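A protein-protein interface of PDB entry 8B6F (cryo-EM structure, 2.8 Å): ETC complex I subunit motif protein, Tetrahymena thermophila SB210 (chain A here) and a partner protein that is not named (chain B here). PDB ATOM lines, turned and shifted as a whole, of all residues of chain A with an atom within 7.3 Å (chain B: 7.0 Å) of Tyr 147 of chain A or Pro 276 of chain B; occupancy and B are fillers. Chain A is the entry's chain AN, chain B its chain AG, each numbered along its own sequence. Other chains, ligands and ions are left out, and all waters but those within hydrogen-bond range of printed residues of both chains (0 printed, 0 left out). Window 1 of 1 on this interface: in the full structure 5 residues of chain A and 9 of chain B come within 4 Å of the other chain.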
ATOM      1  N   TYR A  98       3.732  13.717   8.991  1.00  0.00           N
ATOM      2  CA  TYR A  98       3.828  13.123   7.664  1.00  0.00           C
ATOM      3  C   TYR A  98       5.223  13.323   7.087  1.00  0.00           C
ATOM      4  O   TYR A  98       5.824  12.389   6.543  1.00  0.00           O
ATOM      5  CB  TYR A  98       2.772  13.728   6.739  1.00  0.00           C
ATOM      6  CG  TYR A  98       3.002  13.402   5.285  1.00  0.00           C
ATOM      7  CD1 TYR A  98       2.818  12.112   4.809  1.00  0.00           C
ATOM      8  CD2 TYR A  98       3.401  14.382   4.387  1.00  0.00           C
ATOM      9  CE1 TYR A  98       3.028  11.805   3.483  1.00  0.00           C
ATOM     10  CE2 TYR A  98       3.616  14.085   3.056  1.00  0.00           C
ATOM     11  CZ  TYR A  98       3.428  12.794   2.613  1.00  0.00           C
ATOM     12  OH  TYR A  98       3.636  12.488   1.290  1.00  0.00           O
ATOM     13  N   LYS A 140       4.942   6.495  -6.499  1.00  0.00           N
ATOM     14  CA  LYS A 140       3.680   7.178  -6.250  1.00  0.00           C
ATOM     15  C   LYS A 140       3.776   8.212  -5.138  1.00  0.00           C
ATOM     16  O   LYS A 140       2.907   9.084  -5.047  1.00  0.00           O
ATOM     17  CB  LYS A 140       2.590   6.163  -5.906  1.00  0.00           C
ATOM     18  CG  LYS A 140       2.358   5.127  -6.987  1.00  0.00           C
ATOM     19  CD  LYS A 140       1.292   4.135  -6.577  1.00  0.00           C
ATOM     20  CE  LYS A 140       1.155   3.029  -7.608  1.00  0.00           C
ATOM     21  NZ  LYS A 140       0.133   2.022  -7.212  1.00  0.00           N
ATOM     22  N   GLU A 141       4.804   8.135  -4.292  1.00  0.00           N
ATOM     23  CA  GLU A 141       4.944   9.116  -3.223  1.00  0.00           C
ATOM     24  C   GLU A 141       5.198  10.512  -3.773  1.00  0.00           C
ATOM     25  O   GLU A 141       4.835  11.502  -3.132  1.00  0.00           O
ATOM     26  CB  GLU A 141       6.057   8.700  -2.265  1.00  0.00           C
ATOM     27  CG  GLU A 141       5.740   7.418  -1.510  1.00  0.00           C
ATOM     28  CD  GLU A 141       6.723   7.135  -0.393  1.00  0.00           C
ATOM     29  OE1 GLU A 141       7.750   7.840  -0.307  1.00  0.00           O
ATOM     30  OE2 GLU A 141       6.465   6.210   0.406  1.00  0.00           O
ATOM     31  N   LEU A 142       5.799  10.612  -4.959  1.00  0.00           N
ATOM     32  CA  LEU A 142       6.004  11.919  -5.576  1.00  0.00           C
ATOM     33  C   LEU A 142       4.680  12.642  -5.777  1.00  0.00           C
ATOM     34  O   LEU A 142       4.574  13.846  -5.518  1.00  0.00           O
ATOM     35  CB  LEU A 142       6.737  11.761  -6.907  1.00  0.00           C
ATOM     36  CG  LEU A 142       8.153  11.193  -6.819  1.00  0.00           C
ATOM     37  CD1 LEU A 142       8.663  10.817  -8.197  1.00  0.00           C
ATOM     38  CD2 LEU A 142       9.090  12.191  -6.159  1.00  0.00           C
ATOM     39  N   GLU A 143       3.658  11.926  -6.243  1.00  0.00           N
ATOM     40  CA  GLU A 143       2.333  12.519  -6.380  1.00  0.00           C
ATOM     41  C   GLU A 143       1.625  12.641  -5.037  1.00  0.00           C
ATOM     42  O   GLU A 143       0.866  13.593  -4.829  1.00  0.00           O
ATOM     43  CB  GLU A 143       1.479  11.693  -7.346  1.00  0.00           C
ATOM     44  CG  GLU A 143       1.991  11.678  -8.783  1.00  0.00           C
ATOM     45  CD  GLU A 143       3.219  10.803  -8.971  1.00  0.00           C
ATOM     46  OE1 GLU A 143       3.499   9.969  -8.085  1.00  0.00           O
ATOM     47  OE2 GLU A 143       3.906  10.951 -10.003  1.00  0.00           O
ATOM     48  N   LEU A 144       1.857  11.700  -4.122  1.00  0.00           N
ATOM     49  CA  LEU A 144       1.203  11.758  -2.820  1.00  0.00           C
ATOM     50  C   LEU A 144       1.618  12.992  -2.030  1.00  0.00           C
ATOM     51  O   LEU A 144       0.857  13.465  -1.179  1.00  0.00           O
ATOM     52  CB  LEU A 144       1.521  10.493  -2.023  1.00  0.00           C
ATOM     53  CG  LEU A 144       1.041  10.451  -0.571  1.00  0.00           C
ATOM     54  CD1 LEU A 144      -0.466  10.600  -0.495  1.00  0.00           C
ATOM     55  CD2 LEU A 144       1.487   9.164   0.096  1.00  0.00           C
ATOM     56  N   VAL A 145       2.815  13.525  -2.286  1.00  0.00           N
ATOM     57  CA  VAL A 145       3.301  14.665  -1.509  1.00  0.00           C
ATOM     58  C   VAL A 145       2.353  15.849  -1.652  1.00  0.00           C
ATOM     59  O   VAL A 145       1.972  16.484  -0.662  1.00  0.00           O
ATOM     60  CB  VAL A 145       4.736  15.035  -1.927  1.00  0.00           C
ATOM     61  CG1 VAL A 145       5.118  16.412  -1.405  1.00  0.00           C
ATOM     62  CG2 VAL A 145       5.722  14.009  -1.402  1.00  0.00           C
ATOM     63  N   GLU A 146       1.957  16.165  -2.885  1.00  0.00           N
ATOM     64  CA  GLU A 146       1.082  17.314  -3.094  1.00  0.00           C
ATOM     65  C   GLU A 146      -0.311  17.057  -2.537  1.00  0.00           C
ATOM     66  O   GLU A 146      -0.946  17.969  -1.998  1.00  0.00           O
ATOM     67  CB  GLU A 146       1.011  17.661  -4.579  1.00  0.00           C
ATOM     68  CG  GLU A 146       0.223  18.929  -4.861  1.00  0.00           C
ATOM     69  CD  GLU A 146       0.339  19.381  -6.300  1.00  0.00           C
ATOM     70  OE1 GLU A 146       1.068  18.723  -7.072  1.00  0.00           O
ATOM     71  OE2 GLU A 146      -0.297  20.394  -6.660  1.00  0.00           O
ATOM     72  N   TYR A 147      -0.810  15.827  -2.667  1.00  0.00           N
ATOM     73  CA  TYR A 147      -2.107  15.495  -2.087  1.00  0.00           C
ATOM     74  C   TYR A 147      -2.108  15.722  -0.583  1.00  0.00           C
ATOM     75  O   TYR A 147      -3.044  16.312  -0.031  1.00  0.00           O
ATOM     76  CB  TYR A 147      -2.472  14.045  -2.397  1.00  0.00           C
ATOM     77  CG  TYR A 147      -3.104  13.850  -3.746  1.00  0.00           C
ATOM     78  CD1 TYR A 147      -4.390  14.304  -3.993  1.00  0.00           C
ATOM     79  CD2 TYR A 147      -2.432  13.189  -4.760  1.00  0.00           C
ATOM     80  CE1 TYR A 147      -4.983  14.122  -5.217  1.00  0.00           C
ATOM     81  CE2 TYR A 147      -3.018  13.003  -5.990  1.00  0.00           C
ATOM     82  CZ  TYR A 147      -4.294  13.469  -6.209  1.00  0.00           C
ATOM     83  OH  TYR A 147      -4.878  13.284  -7.432  1.00  0.00           O
ATOM     84  N   MET A 148      -1.060  15.262   0.100  1.00  0.00           N
ATOM     85  CA  MET A 148      -0.979  15.452   1.543  1.00  0.00           C
ATOM     86  C   MET A 148      -0.767  16.915   1.900  1.00  0.00           C
ATOM     87  O   MET A 148      -1.263  17.377   2.933  1.00  0.00           O
ATOM     88  CB  MET A 148       0.142  14.593   2.125  1.00  0.00           C
ATOM     89  CG  MET A 148      -0.146  13.099   2.090  1.00  0.00           C
ATOM     90  SD  MET A 148      -1.614  12.626   3.026  1.00  0.00           S
ATOM     91  CE  MET A 148      -2.839  12.517   1.722  1.00  0.00           C
ATOM     92  N   LYS A 149      -0.040  17.657   1.065  1.00  0.00           N
ATOM     93  CA  LYS A 149       0.119  19.086   1.305  1.00  0.00           C
ATOM     94  C   LYS A 149      -1.229  19.795   1.279  1.00  0.00           C
ATOM     95  O   LYS A 149      -1.493  20.673   2.108  1.00  0.00           O
ATOM     96  CB  LYS A 149       1.063  19.682   0.261  1.00  0.00           C
ATOM     97  CG  LYS A 149       1.180  21.196   0.309  1.00  0.00           C
ATOM     98  CD  LYS A 149       2.206  21.713  -0.691  1.00  0.00           C
ATOM     99  CE  LYS A 149       1.787  21.435  -2.129  1.00  0.00           C
ATOM    100  NZ  LYS A 149       2.736  22.027  -3.115  1.00  0.00           N
ATOM    101  N   HIS A 150      -2.092  19.438   0.326  1.00  0.00           N
ATOM    102  CA  HIS A 150      -3.397  20.084   0.240  1.00  0.00           C
ATOM    103  C   HIS A 150      -4.334  19.601   1.341  1.00  0.00           C
ATOM    104  O   HIS A 150      -5.115  20.389   1.886  1.00  0.00           O
ATOM    105  CB  HIS A 150      -4.008  19.840  -1.138  1.00  0.00           C
ATOM    106  CG  HIS A 150      -3.412  20.690  -2.215  1.00  0.00           C
ATOM    107  ND1 HIS A 150      -2.183  20.422  -2.781  1.00  0.00           N
ATOM    108  CD2 HIS A 150      -3.868  21.811  -2.823  1.00  0.00           C
ATOM    109  CE1 HIS A 150      -1.912  21.338  -3.694  1.00  0.00           C
ATOM    110  NE2 HIS A 150      -2.918  22.193  -3.738  1.00  0.00           N
ATOM    111  N   SER A 151      -4.280  18.310   1.677  1.00  0.00           N
ATOM    112  CA  SER A 151      -5.151  17.792   2.729  1.00  0.00           C
ATOM    113  C   SER A 151      -4.773  18.360   4.090  1.00  0.00           C
ATOM    114  O   SER A 151      -5.648  18.621   4.924  1.00  0.00           O
ATOM    115  CB  SER A 151      -5.094  16.264   2.757  1.00  0.00           C
ATOM    116  OG  SER A 151      -5.717  15.709   1.615  1.00  0.00           O
ATOM    117  N   LYS A 152      -3.479  18.552   4.336  1.00  0.00           N
ATOM    118  CA  LYS A 152      -2.997  19.094   5.600  1.00  0.00           C
ATOM    119  C   LYS A 152      -3.408  18.193   6.757  1.00  0.00           C
ATOM    120  O   LYS A 152      -4.204  18.603   7.611  1.00  0.00           O
ATOM    121  CB  LYS A 152      -3.523  20.514   5.813  1.00  0.00           C
ATOM    122  CG  LYS A 152      -3.152  21.474   4.693  1.00  0.00           C
ATOM    123  CD  LYS A 152      -3.705  22.865   4.946  1.00  0.00           C
ATOM    124  CE  LYS A 152      -3.336  23.808   3.812  1.00  0.00           C
ATOM    125  NZ  LYS A 152      -3.860  25.183   4.035  1.00  0.00           N
ATOM    126  N   PRO A 153      -2.888  16.966   6.826  1.00  0.00           N
ATOM    127  CA  PRO A 153      -3.232  16.089   7.956  1.00  0.00           C
ATOM    128  C   PRO A 153      -2.774  16.618   9.302  1.00  0.00           C
ATOM    129  O   PRO A 153      -3.263  16.144  10.333  1.00  0.00           O
ATOM    130  CB  PRO A 153      -2.536  14.766   7.601  1.00  0.00           C
ATOM    131  CG  PRO A 153      -1.464  15.138   6.644  1.00  0.00           C
ATOM    132  CD  PRO A 153      -1.986  16.306   5.869  1.00  0.00           C
ATOM    133  N   GLU B 273      -5.367   5.604 -14.971  1.00  0.00           N
ATOM    134  CA  GLU B 273      -6.402   6.284 -14.211  1.00  0.00           C
ATOM    135  C   GLU B 273      -6.087   7.770 -14.083  1.00  0.00           C
ATOM    136  O   GLU B 273      -4.939   8.205 -14.197  1.00  0.00           O
ATOM    137  CB  GLU B 273      -6.542   5.665 -12.821  1.00  0.00           C
ATOM    138  CG  GLU B 273      -6.944   4.204 -12.837  1.00  0.00           C
ATOM    139  CD  GLU B 273      -8.307   3.983 -13.460  1.00  0.00           C
ATOM    140  OE1 GLU B 273      -9.135   4.916 -13.425  1.00  0.00           O
ATOM    141  OE2 GLU B 273      -8.547   2.878 -13.988  1.00  0.00           O
ATOM    142  N   GLN B 274      -7.135   8.550 -13.843  1.00  0.00           N
ATOM    143  CA  GLN B 274      -7.005   9.988 -13.676  1.00  0.00           C
ATOM    144  C   GLN B 274      -6.756  10.328 -12.216  1.00  0.00           C
ATOM    145  O   GLN B 274      -7.322   9.704 -11.314  1.00  0.00           O
ATOM    146  CB  GLN B 274      -8.260  10.700 -14.177  1.00  0.00           C
ATOM    147  CG  GLN B 274      -8.494  10.506 -15.659  1.00  0.00           C
ATOM    148  CD  GLN B 274      -9.605  11.377 -16.192  1.00  0.00           C
ATOM    149  OE1 GLN B 274     -10.366  11.972 -15.431  1.00  0.00           O
ATOM    150  NE2 GLN B 274      -9.702  11.461 -17.513  1.00  0.00           N
ATOM    151  N   LEU B 275      -5.908  11.320 -11.991  1.00  0.00           N
ATOM    152  CA  LEU B 275      -5.559  11.698 -10.632  1.00  0.00           C
ATOM    153  C   LEU B 275      -6.801  12.189  -9.894  1.00  0.00           C
ATOM    154  O   LEU B 275      -7.528  13.044 -10.417  1.00  0.00           O
ATOM    155  CB  LEU B 275      -4.484  12.784 -10.654  1.00  0.00           C
ATOM    156  CG  LEU B 275      -3.126  12.381 -11.233  1.00  0.00           C
ATOM    157  CD1 LEU B 275      -2.233  13.595 -11.393  1.00  0.00           C
ATOM    158  CD2 LEU B 275      -2.453  11.343 -10.351  1.00  0.00           C
ATOM    159  N   PRO B 276      -7.081  11.684  -8.688  1.00  0.00           N
ATOM    160  CA  PRO B 276      -8.286  12.118  -7.987  1.00  0.00           C
ATOM    161  C   PRO B 276      -8.203  13.589  -7.625  1.00  0.00           C
ATOM    162  O   PRO B 276      -7.101  14.140  -7.459  1.00  0.00           O
ATOM    163  CB  PRO B 276      -8.307  11.227  -6.732  1.00  0.00           C
ATOM    164  CG  PRO B 276      -6.904  10.825  -6.531  1.00  0.00           C
ATOM    165  CD  PRO B 276      -6.316  10.702  -7.902  1.00  0.00           C
ATOM    166  N   PRO B 277      -9.341  14.270  -7.498  1.00  0.00           N
ATOM    167  CA  PRO B 277      -9.302  15.700  -7.175  1.00  0.00           C
ATOM    168  C   PRO B 277      -8.634  15.960  -5.835  1.00  0.00           C
ATOM    169  O   PRO B 277      -8.735  15.165  -4.898  1.00  0.00           O
ATOM    170  CB  PRO B 277     -10.782  16.100  -7.142  1.00  0.00           C
ATOM    171  CG  PRO B 277     -11.496  15.036  -7.890  1.00  0.00           C
ATOM    172  CD  PRO B 277     -10.720  13.782  -7.664  1.00  0.00           C
ATOM    173  N   LEU B 278      -7.942  17.092  -5.752  1.00  0.00           N
ATOM    174  CA  LEU B 278      -7.411  17.543  -4.476  1.00  0.00           C
ATOM    175  C   LEU B 278      -8.559  17.831  -3.518  1.00  0.00           C
ATOM    176  O   LEU B 278      -9.606  18.346  -3.918  1.00  0.00           O
ATOM    177  CB  LEU B 278      -6.560  18.798  -4.665  1.00  0.00           C
ATOM    178  CG  LEU B 278      -5.374  18.667  -5.621  1.00  0.00           C
ATOM    179  CD1 LEU B 278      -4.837  20.038  -5.982  1.00  0.00           C
ATOM    180  CD2 LEU B 278      -4.283  17.812  -5.006  1.00  0.00           C
ATOM    181  N   GLU B 279      -8.363  17.497  -2.242  1.00  0.00           N
ATOM    182  CA  GLU B 279      -9.429  17.694  -1.270  1.00  0.00           C
ATOM    183  C   GLU B 279      -9.763  19.166  -1.074  1.00  0.00           C
ATOM    184  O   GLU B 279     -10.852  19.480  -0.584  1.00  0.00           O
ATOM    185  CB  GLU B 279      -9.051  17.060   0.067  1.00  0.00           C
ATOM    186  CG  GLU B 279     -10.238  16.871   0.995  1.00  0.00           C
ATOM    187  CD  GLU B 279      -9.885  16.079   2.232  1.00  0.00           C
ATOM    188  OE1 GLU B 279      -8.681  15.856   2.466  1.00  0.00           O
ATOM    189  OE2 GLU B 279     -10.810  15.673   2.968  1.00  0.00           O
ATOM    190  N   GLU B 281     -10.500  21.073  -3.393  1.00  0.00           N
ATOM    191  CA  GLU B 281     -11.546  21.363  -4.360  1.00  0.00           C
ATOM    192  C   GLU B 281     -12.940  21.086  -3.818  1.00  0.00           C
ATOM    193  O   GLU B 281     -13.922  21.449  -4.473  1.00  0.00           O
ATOM    194  CB  GLU B 281     -11.316  20.546  -5.630  1.00  0.00           C
ATOM    195  CG  GLU B 281      -9.951  20.773  -6.262  1.00  0.00           C
ATOM    196  CD  GLU B 281      -9.742  19.943  -7.513  1.00  0.00           C
ATOM    197  OE1 GLU B 281     -10.726  19.360  -8.012  1.00  0.00           O
ATOM    198  OE2 GLU B 281      -8.592  19.871  -7.996  1.00  0.00           O
ATOM    199  N   PHE B 282     -13.053  20.447  -2.657  1.00  0.00           N
ATOM    200  CA  PHE B 282     -14.340  20.176  -2.036  1.00  0.00           C
ATOM    201  C   PHE B 282     -14.735  21.236  -1.017  1.00  0.00           C
ATOM    202  O   PHE B 282     -15.797  21.113  -0.400  1.00  0.00           O
ATOM    203  CB  PHE B 282     -14.325  18.804  -1.352  1.00  0.00           C
ATOM    204  CG  PHE B 282     -13.872  17.679  -2.241  1.00  0.00           C
ATOM    205  CD1 PHE B 282     -13.908  17.797  -3.621  1.00  0.00           C
ATOM    206  CD2 PHE B 282     -13.418  16.494  -1.689  1.00  0.00           C
ATOM    207  CE1 PHE B 282     -13.492  16.758  -4.431  1.00  0.00           C
ATOM    208  CE2 PHE B 282     -13.000  15.453  -2.495  1.00  0.00           C
ATOM    209  CZ  PHE B 282     -13.038  15.585  -3.866  1.00  0.00           C
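Tyr 147 of chain A touches just these residues of chain B: Leu 275 (3.3 Å), Pro 276 (2.4 Å), Pro 277 (3.9 Å) and Leu 278 (3.7 Å).
Of the printed residues of chain A, Pro 276 of chain B touches Tyr 147.
Of the printed residues of chain A, Glu 279 of chain B touches Ser 151 (3.1 Å).
Printed residues of chain A within 4 Å of Pro 277 of chain B: Tyr 147 (3.9 Å).
Printed residues of chain A within 4 Å of Leu 278 of chain B: Tyr 147 and His 150.
The nearest printed residue of chain B that does not touch Ser 151 of chain A is Leu 278 of chain B (6.2 Å).
Of the 9 printed residues of chain B, 5 touch a printed residue of chain A.
Printed residues of chain B that touch a printed residue of chain A: Leu 275, Pro 276, Pro 277, Leu 278 and Glu 279.
Hydrophobic or aromatic side chains of chain B within 4 Å of the printed part of chain A: Leu 275, Pro 276 and Leu 278.
Among the printed residues, 6 pairs touch across the chains.
The side-chain carboxylate of Glu 279 of chain B lies within hydrogen-bond range of the side-chain hydroxyl of Ser 151 of chain A (3.1 Å).
The side-chain hydroxyl of Tyr 147 of chain A sits close to the backbone carbonyl oxygen of Pro 276 of chain B.
OH of Tyr 147 of chain A touches CB of Leu 275 of chain B, at 3.3 Å.
Tyr 147 of chain A touches Pro 277 of chain B.
CD1 of Tyr 147 of chain A touches CD2 of Leu 278 of chain B (3.7 Å).
CD1 of Leu 278 of chain B touches NE2 of His 150 of chain A, 3.7 Å away.
A ring nitrogen (ND1) of His 150 of chain A sits at hydrogen-bond distance from the backbone carbonyl oxygen (O) of Glu 146 of chain A (2.9 Å).
The side-chain hydroxyl of Ser 151 of chain A sits at hydrogen-bond distance from the backbone carbonyl oxygen of Tyr 147 of chain A (3.2 Å).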
